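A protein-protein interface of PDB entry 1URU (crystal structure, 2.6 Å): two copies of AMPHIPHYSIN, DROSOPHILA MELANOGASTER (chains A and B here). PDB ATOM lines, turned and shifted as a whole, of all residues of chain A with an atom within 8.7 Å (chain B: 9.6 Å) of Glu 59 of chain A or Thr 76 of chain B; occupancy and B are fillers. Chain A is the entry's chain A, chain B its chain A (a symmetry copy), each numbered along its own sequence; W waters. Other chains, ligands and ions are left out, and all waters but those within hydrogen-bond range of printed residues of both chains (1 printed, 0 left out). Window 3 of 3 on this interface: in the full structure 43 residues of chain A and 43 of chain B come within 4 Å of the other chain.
NZ of Lys 75 of chain B lies within salt-bridge range of OD2 of Asp 79 of chain B (3.3 Å).
The backbone carbonyl oxygen (O) of Asn 62 of chain A is in hydrogen-bond range of the side-chain sulfur (SG) of Cys 66 of chain A (3.4 Å).
The backbone carbonyl oxygen (O) of Ala 73 of chain B sits at hydrogen-bond distance from the side-chain hydroxyl (OG1) of Thr 76 of chain B, at 3.3 Å.
The side-chain amide oxygen (OD1) of Asn 62 of chain A lies within hydrogen-bond range of the guanidinium group (NH2) of Arg 65 of chain A (3.4 Å).
Water W1 lies within hydrogen-bond range of O of Glu 59 of chain A, ND2 of Asn 62 of chain A, OG1 of Thr 76 of chain B and O of Ala 73 of chain B.
Among the printed residues, pairs that only touch across the chains: Ser 52 of chain A with Ile 84 of chain B, Arg 55 of chain A with Asp 79 of chain B, Leu 56 of chain A with Ser 80 of chain B, Glu 59 of chain A with Leu 77 of chain B, Glu 59 of chain A with Ser 80 of chain B, Phe 60 of chain A with Leu 77 of chain B, Asn 62 of chain A with Ala 73 of chain B, Tyr 63 of chain A with Ser 74 of chain B, Tyr 63 of chain A with Leu 77 of chain B, Cys 66 of chain A with Ala 69 of chain B and Cys 66 of chain A with Ala 73 of chain B.
The side-chain hydroxyl (OG) of Ser 52 of chain A lies within hydrogen-bond range of the side-chain carboxylate (OE1) of Glu 83 of chain B (3.0 Å).
The side-chain hydroxyl of Ser 80 of chain B is in hydrogen-bond range of the guanidinium group of Arg 55 of chain A.
The guanidinium group (NH1) of Arg 55 of chain A lies within salt-bridge range of the side-chain carboxylate (OE2) of Glu 83 of chain B, 3.2 Å away.
The side-chain hydroxyl (OG1) of Thr 76 of chain B sits at hydrogen-bond distance from the side-chain carboxylate (OE1) of Glu 59 of chain A, 2.8 Å away.
Of the 20 printed residues of chain B, 9 touch a printed residue of chain A.
Among the printed residues, Asp or Glu carboxylates within 4 Å of a Lys or Arg side-chain nitrogen of the other chain: Arg 55 of chain A with Glu 83 of chain B (3.2 Å).
Of the printed residues of chain B, Leu 56 of chain A touches Ser 80.
Glu 59 of chain A touches three residues of chain B.
Of the printed residues of chain B, Phe 60 of chain A touches Leu 77.
Of chain A, only Glu 59 comes within 4 Å of Thr 76 of chain B.
Printed residues of chain A within 4 Å of Glu 83 of chain B: Ser 52 (3.0 Å) and Arg 55 (3.2 Å).
The nearest printed residue of chain A that does not touch Ser 80 of chain B is Ser 52 of chain A (5.7 Å).
No position is printed for both chains.
Of the 15 pairs that touch across the chains among the printed residues, none has its exchanged pair printed and touching as well.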
ATOM      1  N   SER A  52      13.850 -12.479  10.547  1.00  0.00           N
ATOM      2  CA  SER A  52      13.413 -13.633   9.743  1.00  0.00           C
ATOM      3  C   SER A  52      14.176 -14.914  10.115  1.00  0.00           C
ATOM      4  O   SER A  52      13.602 -15.987  10.109  1.00  0.00           O
ATOM      5  CB  SER A  52      13.571 -13.365   8.232  1.00  0.00           C
ATOM      6  OG  SER A  52      12.723 -12.321   7.771  1.00  0.00           O
ATOM      7  N   ALA A  53      15.458 -14.791  10.454  1.00  0.00           N
ATOM      8  CA  ALA A  53      16.252 -15.948  10.868  1.00  0.00           C
ATOM      9  C   ALA A  53      15.916 -16.405  12.298  1.00  0.00           C
ATOM     10  O   ALA A  53      15.937 -17.601  12.580  1.00  0.00           O
ATOM     11  CB  ALA A  53      17.740 -15.657  10.735  1.00  0.00           C
ATOM     12  N   ASN A  54      15.609 -15.451  13.185  1.00  0.00           N
ATOM     13  CA  ASN A  54      15.205 -15.745  14.566  1.00  0.00           C
ATOM     14  C   ASN A  54      13.859 -16.475  14.601  1.00  0.00           C
ATOM     15  O   ASN A  54      13.653 -17.433  15.382  1.00  0.00           O
ATOM     16  CB  ASN A  54      15.120 -14.457  15.382  1.00  0.00           C
ATOM     17  CG  ASN A  54      16.500 -13.905  15.773  1.00  0.00           C
ATOM     18  OD1 ASN A  54      16.603 -12.834  16.344  1.00  0.00           O
ATOM     19  ND2 ASN A  54      17.545 -14.648  15.478  1.00  0.00           N
ATOM     20  N   ARG A  55      12.961 -16.032  13.724  1.00  0.00           N
ATOM     21  CA  ARG A  55      11.678 -16.677  13.553  1.00  0.00           C
ATOM     22  C   ARG A  55      11.849 -18.097  12.975  1.00  0.00           C
ATOM     23  O   ARG A  55      11.144 -19.025  13.383  1.00  0.00           O
ATOM     24  CB  ARG A  55      10.775 -15.820  12.664  1.00  0.00           C
ATOM     25  CG  ARG A  55       9.512 -16.486  12.215  1.00  0.00           C
ATOM     26  CD  ARG A  55       8.676 -15.652  11.258  1.00  0.00           C
ATOM     27  NE  ARG A  55       7.371 -16.261  11.019  1.00  0.00           N
ATOM     28  CZ  ARG A  55       6.433 -15.787  10.202  1.00  0.00           C
ATOM     29  NH1 ARG A  55       6.613 -14.657   9.526  1.00  0.00           N
ATOM     30  NH2 ARG A  55       5.294 -16.462  10.069  1.00  0.00           N
ATOM     31  N   LEU A  56      12.763 -18.282  12.028  1.00  0.00           N
ATOM     32  CA  LEU A  56      12.923 -19.594  11.415  1.00  0.00           C
ATOM     33  C   LEU A  56      13.475 -20.577  12.439  1.00  0.00           C
ATOM     34  O   LEU A  56      13.031 -21.716  12.516  1.00  0.00           O
ATOM     35  CB  LEU A  56      13.846 -19.526  10.208  1.00  0.00           C
ATOM     36  CG  LEU A  56      13.907 -20.791   9.357  1.00  0.00           C
ATOM     37  CD1 LEU A  56      12.549 -21.070   8.749  1.00  0.00           C
ATOM     38  CD2 LEU A  56      14.976 -20.632   8.264  1.00  0.00           C
ATOM     39  N   GLN A  57      14.427 -20.106  13.234  1.00  0.00           N
ATOM     40  CA  GLN A  57      15.054 -20.915  14.268  1.00  0.00           C
ATOM     41  C   GLN A  57      14.032 -21.281  15.359  1.00  0.00           C
ATOM     42  O   GLN A  57      13.958 -22.416  15.783  1.00  0.00           O
ATOM     43  CB  GLN A  57      16.255 -20.173  14.851  1.00  0.00           C
ATOM     44  CG  GLN A  57      17.052 -20.906  15.890  1.00  0.00           C
ATOM     45  CD  GLN A  57      18.079 -20.012  16.550  1.00  0.00           C
ATOM     46  OE1 GLN A  57      17.770 -18.883  16.961  1.00  0.00           O
ATOM     47  NE2 GLN A  57      19.299 -20.494  16.643  1.00  0.00           N
ATOM     48  N   LYS A  58      13.229 -20.316  15.772  1.00  0.00           N
ATOM     49  CA  LYS A  58      12.141 -20.554  16.716  1.00  0.00           C
ATOM     50  C   LYS A  58      11.212 -21.668  16.212  1.00  0.00           C
ATOM     51  O   LYS A  58      11.106 -22.719  16.841  1.00  0.00           O
ATOM     52  CB  LYS A  58      11.363 -19.247  16.940  1.00  0.00           C
ATOM     53  CG  LYS A  58      10.313 -19.311  18.009  1.00  0.00           C
ATOM     54  CD  LYS A  58       9.130 -18.361  17.740  1.00  0.00           C
ATOM     55  CE  LYS A  58       8.205 -18.247  18.968  1.00  0.00           C
ATOM     56  NZ  LYS A  58       8.736 -17.274  19.988  1.00  0.00           N
ATOM     57  N   GLU A  59      10.575 -21.444  15.070  1.00  0.00           N
ATOM     58  CA  GLU A  59       9.621 -22.405  14.524  1.00  0.00           C
ATOM     59  C   GLU A  59      10.212 -23.769  14.258  1.00  0.00           C
ATOM     60  O   GLU A  59       9.553 -24.774  14.462  1.00  0.00           O
ATOM     61  CB  GLU A  59       9.000 -21.901  13.219  1.00  0.00           C
ATOM     62  CG  GLU A  59       8.296 -20.556  13.325  1.00  0.00           C
ATOM     63  CD  GLU A  59       7.302 -20.506  14.467  1.00  0.00           C
ATOM     64  OE1 GLU A  59       6.634 -21.539  14.745  1.00  0.00           O
ATOM     65  OE2 GLU A  59       7.205 -19.422  15.082  1.00  0.00           O
ATOM     66  N   PHE A  60      11.453 -23.805  13.796  1.00  0.00           N
ATOM     67  CA  PHE A  60      12.088 -25.059  13.471  1.00  0.00           C
ATOM     68  C   PHE A  60      12.407 -25.821  14.756  1.00  0.00           C
ATOM     69  O   PHE A  60      12.334 -27.035  14.796  1.00  0.00           O
ATOM     70  CB  PHE A  60      13.356 -24.852  12.622  1.00  0.00           C
ATOM     71  CG  PHE A  60      13.932 -26.124  12.143  1.00  0.00           C
ATOM     72  CD1 PHE A  60      13.269 -26.864  11.195  1.00  0.00           C
ATOM     73  CD2 PHE A  60      15.058 -26.650  12.723  1.00  0.00           C
ATOM     74  CE1 PHE A  60      13.771 -28.087  10.764  1.00  0.00           C
ATOM     75  CE2 PHE A  60      15.568 -27.880  12.312  1.00  0.00           C
ATOM     76  CZ  PHE A  60      14.919 -28.603  11.336  1.00  0.00           C
ATOM     77  N   ASN A  61      12.769 -25.104  15.808  1.00  0.00           N
ATOM     78  CA  ASN A  61      13.005 -25.739  17.097  1.00  0.00           C
ATOM     79  C   ASN A  61      11.700 -26.280  17.678  1.00  0.00           C
ATOM     80  O   ASN A  61      11.687 -27.301  18.346  1.00  0.00           O
ATOM     81  CB  ASN A  61      13.707 -24.786  18.086  1.00  0.00           C
ATOM     82  CG  ASN A  61      15.224 -24.813  17.941  1.00  0.00           C
ATOM     83  OD1 ASN A  61      15.881 -23.781  17.951  1.00  0.00           O
ATOM     84  ND2 ASN A  61      15.786 -25.995  17.804  1.00  0.00           N
ATOM     85  N   ASN A  62      10.608 -25.590  17.395  1.00  0.00           N
ATOM     86  CA  ASN A  62       9.292 -26.050  17.796  1.00  0.00           C
ATOM     87  C   ASN A  62       8.937 -27.322  17.010  1.00  0.00           C
ATOM     88  O   ASN A  62       8.426 -28.265  17.576  1.00  0.00           O
ATOM     89  CB  ASN A  62       8.256 -24.937  17.601  1.00  0.00           C
ATOM     90  CG  ASN A  62       6.867 -25.362  18.024  1.00  0.00           C
ATOM     91  OD1 ASN A  62       6.654 -25.742  19.178  1.00  0.00           O
ATOM     92  ND2 ASN A  62       5.920 -25.330  17.093  1.00  0.00           N
ATOM     93  N   TYR A  63       9.282 -27.348  15.720  1.00  0.00           N
ATOM     94  CA  TYR A  63       9.039 -28.495  14.850  1.00  0.00           C
ATOM     95  C   TYR A  63       9.800 -29.711  15.324  1.00  0.00           C
ATOM     96  O   TYR A  63       9.258 -30.799  15.367  1.00  0.00           O
ATOM     97  CB  TYR A  63       9.468 -28.166  13.444  1.00  0.00           C
ATOM     98  CG  TYR A  63       9.210 -29.237  12.420  1.00  0.00           C
ATOM     99  CD1 TYR A  63       7.916 -29.625  12.111  1.00  0.00           C
ATOM    100  CD2 TYR A  63      10.261 -29.836  11.723  1.00  0.00           C
ATOM    101  CE1 TYR A  63       7.655 -30.594  11.139  1.00  0.00           C
ATOM    102  CE2 TYR A  63      10.015 -30.816  10.745  1.00  0.00           C
ATOM    103  CZ  TYR A  63       8.699 -31.173  10.458  1.00  0.00           C
ATOM    104  OH  TYR A  63       8.427 -32.108   9.514  1.00  0.00           O
ATOM    105  N   ILE A  64      11.047 -29.525  15.710  1.00  0.00           N
ATOM    106  CA  ILE A  64      11.870 -30.652  16.115  1.00  0.00           C
ATOM    107  C   ILE A  64      11.290 -31.363  17.341  1.00  0.00           C
ATOM    108  O   ILE A  64      11.131 -32.576  17.334  1.00  0.00           O
ATOM    109  CB  ILE A  64      13.284 -30.207  16.456  1.00  0.00           C
ATOM    110  CG1 ILE A  64      13.948 -29.529  15.259  1.00  0.00           C
ATOM    111  CG2 ILE A  64      14.080 -31.409  17.002  1.00  0.00           C
ATOM    112  CD1 ILE A  64      15.091 -30.290  14.680  1.00  0.00           C
ATOM    113  N   ARG A  65      11.015 -30.637  18.416  1.00  0.00           N
ATOM    114  CA  ARG A  65      10.456 -31.324  19.572  1.00  0.00           C
ATOM    115  C   ARG A  65       9.049 -31.861  19.274  1.00  0.00           C
ATOM    116  O   ARG A  65       8.643 -32.863  19.838  1.00  0.00           O
ATOM    117  CB  ARG A  65      10.517 -30.475  20.861  1.00  0.00           C
ATOM    118  CG  ARG A  65       9.674 -29.257  20.880  1.00  0.00           C
ATOM    119  CD  ARG A  65       9.036 -28.929  22.248  1.00  0.00           C
ATOM    120  NE  ARG A  65       7.841 -28.121  21.992  1.00  0.00           N
ATOM    121  CZ  ARG A  65       6.591 -28.530  22.103  1.00  0.00           C
ATOM    122  NH1 ARG A  65       6.293 -29.752  22.559  1.00  0.00           N
ATOM    123  NH2 ARG A  65       5.623 -27.689  21.772  1.00  0.00           N
ATOM    124  N   CYS A  66       8.312 -31.241  18.365  1.00  0.00           N
ATOM    125  CA  CYS A  66       7.025 -31.808  18.019  1.00  0.00           C
ATOM    126  C   CYS A  66       7.193 -33.129  17.275  1.00  0.00           C
ATOM    127  O   CYS A  66       6.410 -34.052  17.470  1.00  0.00           O
ATOM    128  CB  CYS A  66       6.153 -30.807  17.272  1.00  0.00           C
ATOM    129  SG  CYS A  66       5.448 -29.613  18.439  1.00  0.00           S
ATOM    130  N   VAL A  67       8.247 -33.210  16.470  1.00  0.00           N
ATOM    131  CA  VAL A  67       8.644 -34.414  15.748  1.00  0.00           C
ATOM    132  C   VAL A  67       9.118 -35.506  16.719  1.00  0.00           C
ATOM    133  O   VAL A  67       8.665 -36.649  16.650  1.00  0.00           O
ATOM    134  CB  VAL A  67       9.827 -34.110  14.753  1.00  0.00           C
ATOM    135  CG1 VAL A  67      10.375 -35.389  14.187  1.00  0.00           C
ATOM    136  CG2 VAL A  67       9.412 -33.120  13.627  1.00  0.00           C
ATOM    137  N   LEU A 118      19.630 -28.222  11.559  1.00  0.00           N
ATOM    138  CA  LEU A 118      19.517 -27.271  12.661  1.00  0.00           C
ATOM    139  C   LEU A 118      20.781 -26.488  12.885  1.00  0.00           C
ATOM    140  O   LEU A 118      20.686 -25.285  13.056  1.00  0.00           O
ATOM    141  CB  LEU A 118      19.124 -27.959  13.971  1.00  0.00           C
ATOM    142  CG  LEU A 118      19.176 -27.081  15.228  1.00  0.00           C
ATOM    143  CD1 LEU A 118      18.112 -25.996  15.188  1.00  0.00           C
ATOM    144  CD2 LEU A 118      19.004 -27.915  16.462  1.00  0.00           C
ATOM    145  N   LEU A 121      21.569 -23.598  10.867  1.00  0.00           N
ATOM    146  CA  LEU A 121      20.566 -22.553  11.134  1.00  0.00           C
ATOM    147  C   LEU A 121      20.936 -21.739  12.353  1.00  0.00           C
ATOM    148  O   LEU A 121      20.766 -20.521  12.353  1.00  0.00           O
ATOM    149  CB  LEU A 121      19.178 -23.154  11.301  1.00  0.00           C
ATOM    150  CG  LEU A 121      17.978 -22.235  11.562  1.00  0.00           C
ATOM    151  CD1 LEU A 121      17.872 -21.073  10.573  1.00  0.00           C
ATOM    152  CD2 LEU A 121      16.684 -23.082  11.588  1.00  0.00           C
ATOM    153  N   ARG B  68      -1.541 -34.126  15.737  1.00  0.00           N
ATOM    154  CA  ARG B  68      -2.200 -32.833  15.703  1.00  0.00           C
ATOM    155  C   ARG B  68      -1.178 -31.738  15.974  1.00  0.00           C
ATOM    156  O   ARG B  68      -1.045 -30.805  15.188  1.00  0.00           O
ATOM    157  CB  ARG B  68      -3.344 -32.768  16.739  1.00  0.00           C
ATOM    158  CG  ARG B  68      -4.746 -32.835  16.130  1.00  0.00           C
ATOM    159  CD  ARG B  68      -5.838 -33.492  17.007  1.00  0.00           C
ATOM    160  NE  ARG B  68      -6.711 -34.351  16.191  1.00  0.00           N
ATOM    161  CZ  ARG B  68      -7.947 -34.772  16.524  1.00  0.00           C
ATOM    162  NH1 ARG B  68      -8.507 -34.416  17.680  1.00  0.00           N
ATOM    163  NH2 ARG B  68      -8.637 -35.545  15.677  1.00  0.00           N
ATOM    164  N   ALA B  69      -0.441 -31.864  17.069  1.00  0.00           N
ATOM    165  CA  ALA B  69       0.587 -30.877  17.411  1.00  0.00           C
ATOM    166  C   ALA B  69       1.683 -30.773  16.335  1.00  0.00           C
ATOM    167  O   ALA B  69       2.235 -29.685  16.115  1.00  0.00           O
ATOM    168  CB  ALA B  69       1.208 -31.208  18.751  1.00  0.00           C
ATOM    169  N   ALA B  70       1.994 -31.890  15.677  1.00  0.00           N
ATOM    170  CA  ALA B  70       2.990 -31.904  14.606  1.00  0.00           C
ATOM    171  C   ALA B  70       2.501 -31.145  13.354  1.00  0.00           C
ATOM    172  O   ALA B  70       3.262 -30.412  12.722  1.00  0.00           O
ATOM    173  CB  ALA B  70       3.374 -33.353  14.250  1.00  0.00           C
ATOM    174  N   GLN B  71       1.224 -31.363  13.018  1.00  0.00           N
ATOM    175  CA  GLN B  71       0.518 -30.637  11.974  1.00  0.00           C
ATOM    176  C   GLN B  71       0.644 -29.127  12.203  1.00  0.00           C
ATOM    177  O   GLN B  71       1.054 -28.369  11.304  1.00  0.00           O
ATOM    178  CB  GLN B  71      -0.953 -31.057  12.000  1.00  0.00           C
ATOM    179  CG  GLN B  71      -1.896 -30.230  11.109  1.00  0.00           C
ATOM    180  CD  GLN B  71      -3.355 -30.633  11.239  1.00  0.00           C
ATOM    181  OE1 GLN B  71      -3.757 -31.195  12.253  1.00  0.00           O
ATOM    182  NE2 GLN B  71      -4.146 -30.327  10.220  1.00  0.00           N
ATOM    183  N   ALA B  72       0.291 -28.714  13.418  1.00  0.00           N
ATOM    184  CA  ALA B  72       0.377 -27.327  13.843  1.00  0.00           C
ATOM    185  C   ALA B  72       1.773 -26.778  13.681  1.00  0.00           C
ATOM    186  O   ALA B  72       1.915 -25.663  13.235  1.00  0.00           O
ATOM    187  CB  ALA B  72      -0.055 -27.172  15.287  1.00  0.00           C
ATOM    188  N   ALA B  73       2.795 -27.546  14.046  1.00  0.00           N
ATOM    189  CA  ALA B  73       4.160 -27.046  14.017  1.00  0.00           C
ATOM    190  C   ALA B  73       4.691 -26.998  12.598  1.00  0.00           C
ATOM    191  O   ALA B  73       5.455 -26.109  12.275  1.00  0.00           O
ATOM    192  CB  ALA B  73       5.073 -27.899  14.889  1.00  0.00           C
ATOM    193  N   SER B  74       4.263 -27.927  11.746  1.00  0.00           N
ATOM    194  CA  SER B  74       4.697 -27.970  10.356  1.00  0.00           C
ATOM    195  C   SER B  74       4.152 -26.759   9.599  1.00  0.00           C
ATOM    196  O   SER B  74       4.759 -26.279   8.630  1.00  0.00           O
ATOM    197  CB  SER B  74       4.203 -29.265   9.706  1.00  0.00           C
ATOM    198  OG  SER B  74       4.553 -29.332   8.333  1.00  0.00           O
ATOM    199  N   LYS B  75       3.007 -26.270  10.082  1.00  0.00           N
ATOM    200  CA  LYS B  75       2.243 -25.195   9.481  1.00  0.00           C
ATOM    201  C   LYS B  75       2.922 -23.878   9.817  1.00  0.00           C
ATOM    202  O   LYS B  75       3.225 -23.093   8.920  1.00  0.00           O
ATOM    203  CB  LYS B  75       0.805 -25.227  10.036  1.00  0.00           C
ATOM    204  CG  LYS B  75      -0.293 -24.536   9.185  1.00  0.00           C
ATOM    205  CD  LYS B  75      -0.216 -23.020   9.261  1.00  0.00           C
ATOM    206  CE  LYS B  75      -1.574 -22.343   9.184  1.00  0.00           C
ATOM    207  NZ  LYS B  75      -1.600 -21.113  10.073  1.00  0.00           N
ATOM    208  N   THR B  76       3.178 -23.631  11.099  1.00  0.00           N
ATOM    209  CA  THR B  76       3.857 -22.395  11.488  1.00  0.00           C
ATOM    210  C   THR B  76       5.289 -22.349  10.945  1.00  0.00           C
ATOM    211  O   THR B  76       5.822 -21.258  10.753  1.00  0.00           O
ATOM    212  CB  THR B  76       3.916 -22.189  13.013  1.00  0.00           C
ATOM    213  OG1 THR B  76       4.741 -23.198  13.603  1.00  0.00           O
ATOM    214  CG2 THR B  76       2.556 -22.350  13.672  1.00  0.00           C
ATOM    215  N   LEU B  77       5.907 -23.514  10.704  1.00  0.00           N
ATOM    216  CA  LEU B  77       7.270 -23.566  10.154  1.00  0.00           C
ATOM    217  C   LEU B  77       7.228 -23.284   8.687  1.00  0.00           C
ATOM    218  O   LEU B  77       8.096 -22.620   8.167  1.00  0.00           O
ATOM    219  CB  LEU B  77       7.962 -24.925  10.382  1.00  0.00           C
ATOM    220  CG  LEU B  77       9.299 -25.174   9.665  1.00  0.00           C
ATOM    221  CD1 LEU B  77      10.327 -24.176  10.121  1.00  0.00           C
ATOM    222  CD2 LEU B  77       9.822 -26.575   9.890  1.00  0.00           C
ATOM    223  N   MET B  78       6.235 -23.823   8.002  1.00  0.00           N
ATOM    224  CA  MET B  78       6.128 -23.616   6.554  1.00  0.00           C
ATOM    225  C   MET B  78       5.713 -22.179   6.263  1.00  0.00           C
ATOM    226  O   MET B  78       6.088 -21.617   5.254  1.00  0.00           O
ATOM    227  CB  MET B  78       5.168 -24.634   5.945  1.00  0.00           C
ATOM    228  CG  MET B  78       5.763 -26.027   5.938  1.00  0.00           C
ATOM    229  SD  MET B  78       7.492 -26.157   4.902  1.00  0.00           S
ATOM    230  CE  MET B  78       6.778 -25.584   3.226  1.00  0.00           C
ATOM    231  N   ASP B  79       4.988 -21.581   7.198  1.00  0.00           N
ATOM    232  CA  ASP B  79       4.559 -20.206   7.084  1.00  0.00           C
ATOM    233  C   ASP B  79       5.780 -19.332   7.179  1.00  0.00           C
ATOM    234  O   ASP B  79       5.792 -18.244   6.637  1.00  0.00           O
ATOM    235  CB  ASP B  79       3.592 -19.829   8.226  1.00  0.00           C
ATOM    236  CG  ASP B  79       2.179 -20.366   8.029  1.00  0.00           C
ATOM    237  OD1 ASP B  79       1.888 -21.017   6.992  1.00  0.00           O
ATOM    238  OD2 ASP B  79       1.297 -20.171   8.900  1.00  0.00           O
ATOM    239  N   SER B  80       6.783 -19.799   7.914  1.00  0.00           N
ATOM    240  CA  SER B  80       8.080 -19.126   7.997  1.00  0.00           C
ATOM    241  C   SER B  80       8.897 -19.262   6.747  1.00  0.00           C
ATOM    242  O   SER B  80       9.494 -18.295   6.317  1.00  0.00           O
ATOM    243  CB  SER B  80       8.920 -19.697   9.111  1.00  0.00           C
ATOM    244  OG  SER B  80       8.738 -18.903  10.232  1.00  0.00           O
ATOM    245  N   VAL B  81       8.975 -20.475   6.209  1.00  0.00           N
ATOM    246  CA  VAL B  81       9.752 -20.721   5.018  1.00  0.00           C
ATOM    247  C   VAL B  81       9.154 -19.857   3.915  1.00  0.00           C
ATOM    248  O   VAL B  81       9.889 -19.250   3.133  1.00  0.00           O
ATOM    249  CB  VAL B  81       9.709 -22.185   4.568  1.00  0.00           C
ATOM    250  CG1 VAL B  81      10.364 -22.323   3.219  1.00  0.00           C
ATOM    251  CG2 VAL B  81      10.395 -23.096   5.579  1.00  0.00           C
ATOM    252  N   CYS B  82       7.821 -19.795   3.873  1.00  0.00           N
ATOM    253  CA  CYS B  82       7.124 -18.995   2.878  1.00  0.00           C
ATOM    254  C   CYS B  82       7.431 -17.511   3.098  1.00  0.00           C
ATOM    255  O   CYS B  82       7.655 -16.798   2.133  1.00  0.00           O
ATOM    256  CB  CYS B  82       5.620 -19.283   2.890  1.00  0.00           C
ATOM    257  SG  CYS B  82       5.145 -20.876   2.123  1.00  0.00           S
ATOM    258  N   GLU B  83       7.506 -17.058   4.351  1.00  0.00           N
ATOM    259  CA  GLU B  83       7.828 -15.648   4.661  1.00  0.00           C
ATOM    260  C   GLU B  83       9.248 -15.208   4.231  1.00  0.00           C
ATOM    261  O   GLU B  83       9.426 -14.129   3.652  1.00  0.00           O
ATOM    262  CB  GLU B  83       7.644 -15.365   6.168  1.00  0.00           C
ATOM    263  CG  GLU B  83       7.833 -13.898   6.586  1.00  0.00           C
ATOM    264  CD  GLU B  83       9.228 -13.583   7.184  1.00  0.00           C
ATOM    265  OE1 GLU B  83      10.164 -13.259   6.402  1.00  0.00           O
ATOM    266  OE2 GLU B  83       9.399 -13.642   8.436  1.00  0.00           O
ATOM    267  N   ILE B  84      10.248 -16.035   4.540  1.00  0.00           N
ATOM    268  CA  ILE B  84      11.656 -15.706   4.346  1.00  0.00           C
ATOM    269  C   ILE B  84      12.118 -15.923   2.898  1.00  0.00           C
ATOM    270  O   ILE B  84      13.187 -15.472   2.503  1.00  0.00           O
ATOM    271  CB  ILE B  84      12.515 -16.556   5.322  1.00  0.00           C
ATOM    272  CG1 ILE B  84      13.950 -16.038   5.377  1.00  0.00           C
ATOM    273  CG2 ILE B  84      12.506 -18.051   4.932  1.00  0.00           C
ATOM    274  CD1 ILE B  84      14.682 -16.428   6.620  1.00  0.00           C
ATOM    275  N   THR B  99       3.161 -25.818  -0.377  1.00  0.00           N
ATOM    276  CA  THR B  99       2.945 -25.677   1.048  1.00  0.00           C
ATOM    277  C   THR B  99       1.479 -25.843   1.430  1.00  0.00           C
ATOM    278  O   THR B  99       1.171 -26.535   2.394  1.00  0.00           O
ATOM    279  CB  THR B  99       3.434 -24.290   1.449  1.00  0.00           C
ATOM    280  OG1 THR B  99       4.851 -24.339   1.579  1.00  0.00           O
ATOM    281  CG2 THR B  99       2.904 -23.837   2.819  1.00  0.00           C
ATOM    282  N   GLU B 103      -0.669 -28.619   3.905  1.00  0.00           N
ATOM    283  CA  GLU B 103      -1.614 -28.334   4.980  1.00  0.00           C
ATOM    284  C   GLU B 103      -2.813 -29.260   4.906  1.00  0.00           C
ATOM    285  O   GLU B 103      -3.335 -29.680   5.931  1.00  0.00           O
ATOM    286  CB  GLU B 103      -2.092 -26.872   4.936  1.00  0.00           C
ATOM    287  CG  GLU B 103      -1.114 -25.869   5.546  1.00  0.00           C
ATOM    288  CD  GLU B 103      -1.693 -24.460   5.659  1.00  0.00           C
ATOM    289  OE1 GLU B 103      -2.841 -24.304   6.131  1.00  0.00           O
ATOM    290  OE2 GLU B 103      -1.001 -23.493   5.276  1.00  0.00           O
ATOM    291  N   TRP B 106      -2.013 -33.079   5.715  1.00  0.00           N
ATOM    292  CA  TRP B 106      -1.925 -33.195   7.153  1.00  0.00           C
ATOM    293  C   TRP B 106      -3.330 -33.202   7.743  1.00  0.00           C
ATOM    294  O   TRP B 106      -3.579 -33.865   8.746  1.00  0.00           O
ATOM    295  CB  TRP B 106      -1.124 -32.041   7.763  1.00  0.00           C
ATOM    296  CG  TRP B 106       0.388 -32.265   7.908  1.00  0.00           C
ATOM    297  CD1 TRP B 106       1.376 -31.821   7.058  1.00  0.00           C
ATOM    298  CD2 TRP B 106       1.063 -32.953   8.971  1.00  0.00           C
ATOM    299  NE1 TRP B 106       2.608 -32.186   7.538  1.00  0.00           N
ATOM    300  CE2 TRP B 106       2.452 -32.882   8.706  1.00  0.00           C
ATOM    301  CE3 TRP B 106       0.637 -33.616  10.133  1.00  0.00           C
ATOM    302  CZ2 TRP B 106       3.418 -33.445   9.560  1.00  0.00           C
ATOM    303  CZ3 TRP B 106       1.603 -34.180  10.983  1.00  0.00           C
ATOM    304  CH2 TRP B 106       2.974 -34.087  10.690  1.00  0.00           C
HETATM  305  O   HOH W   1       6.841 -24.795  14.523  1.00  0.00           O
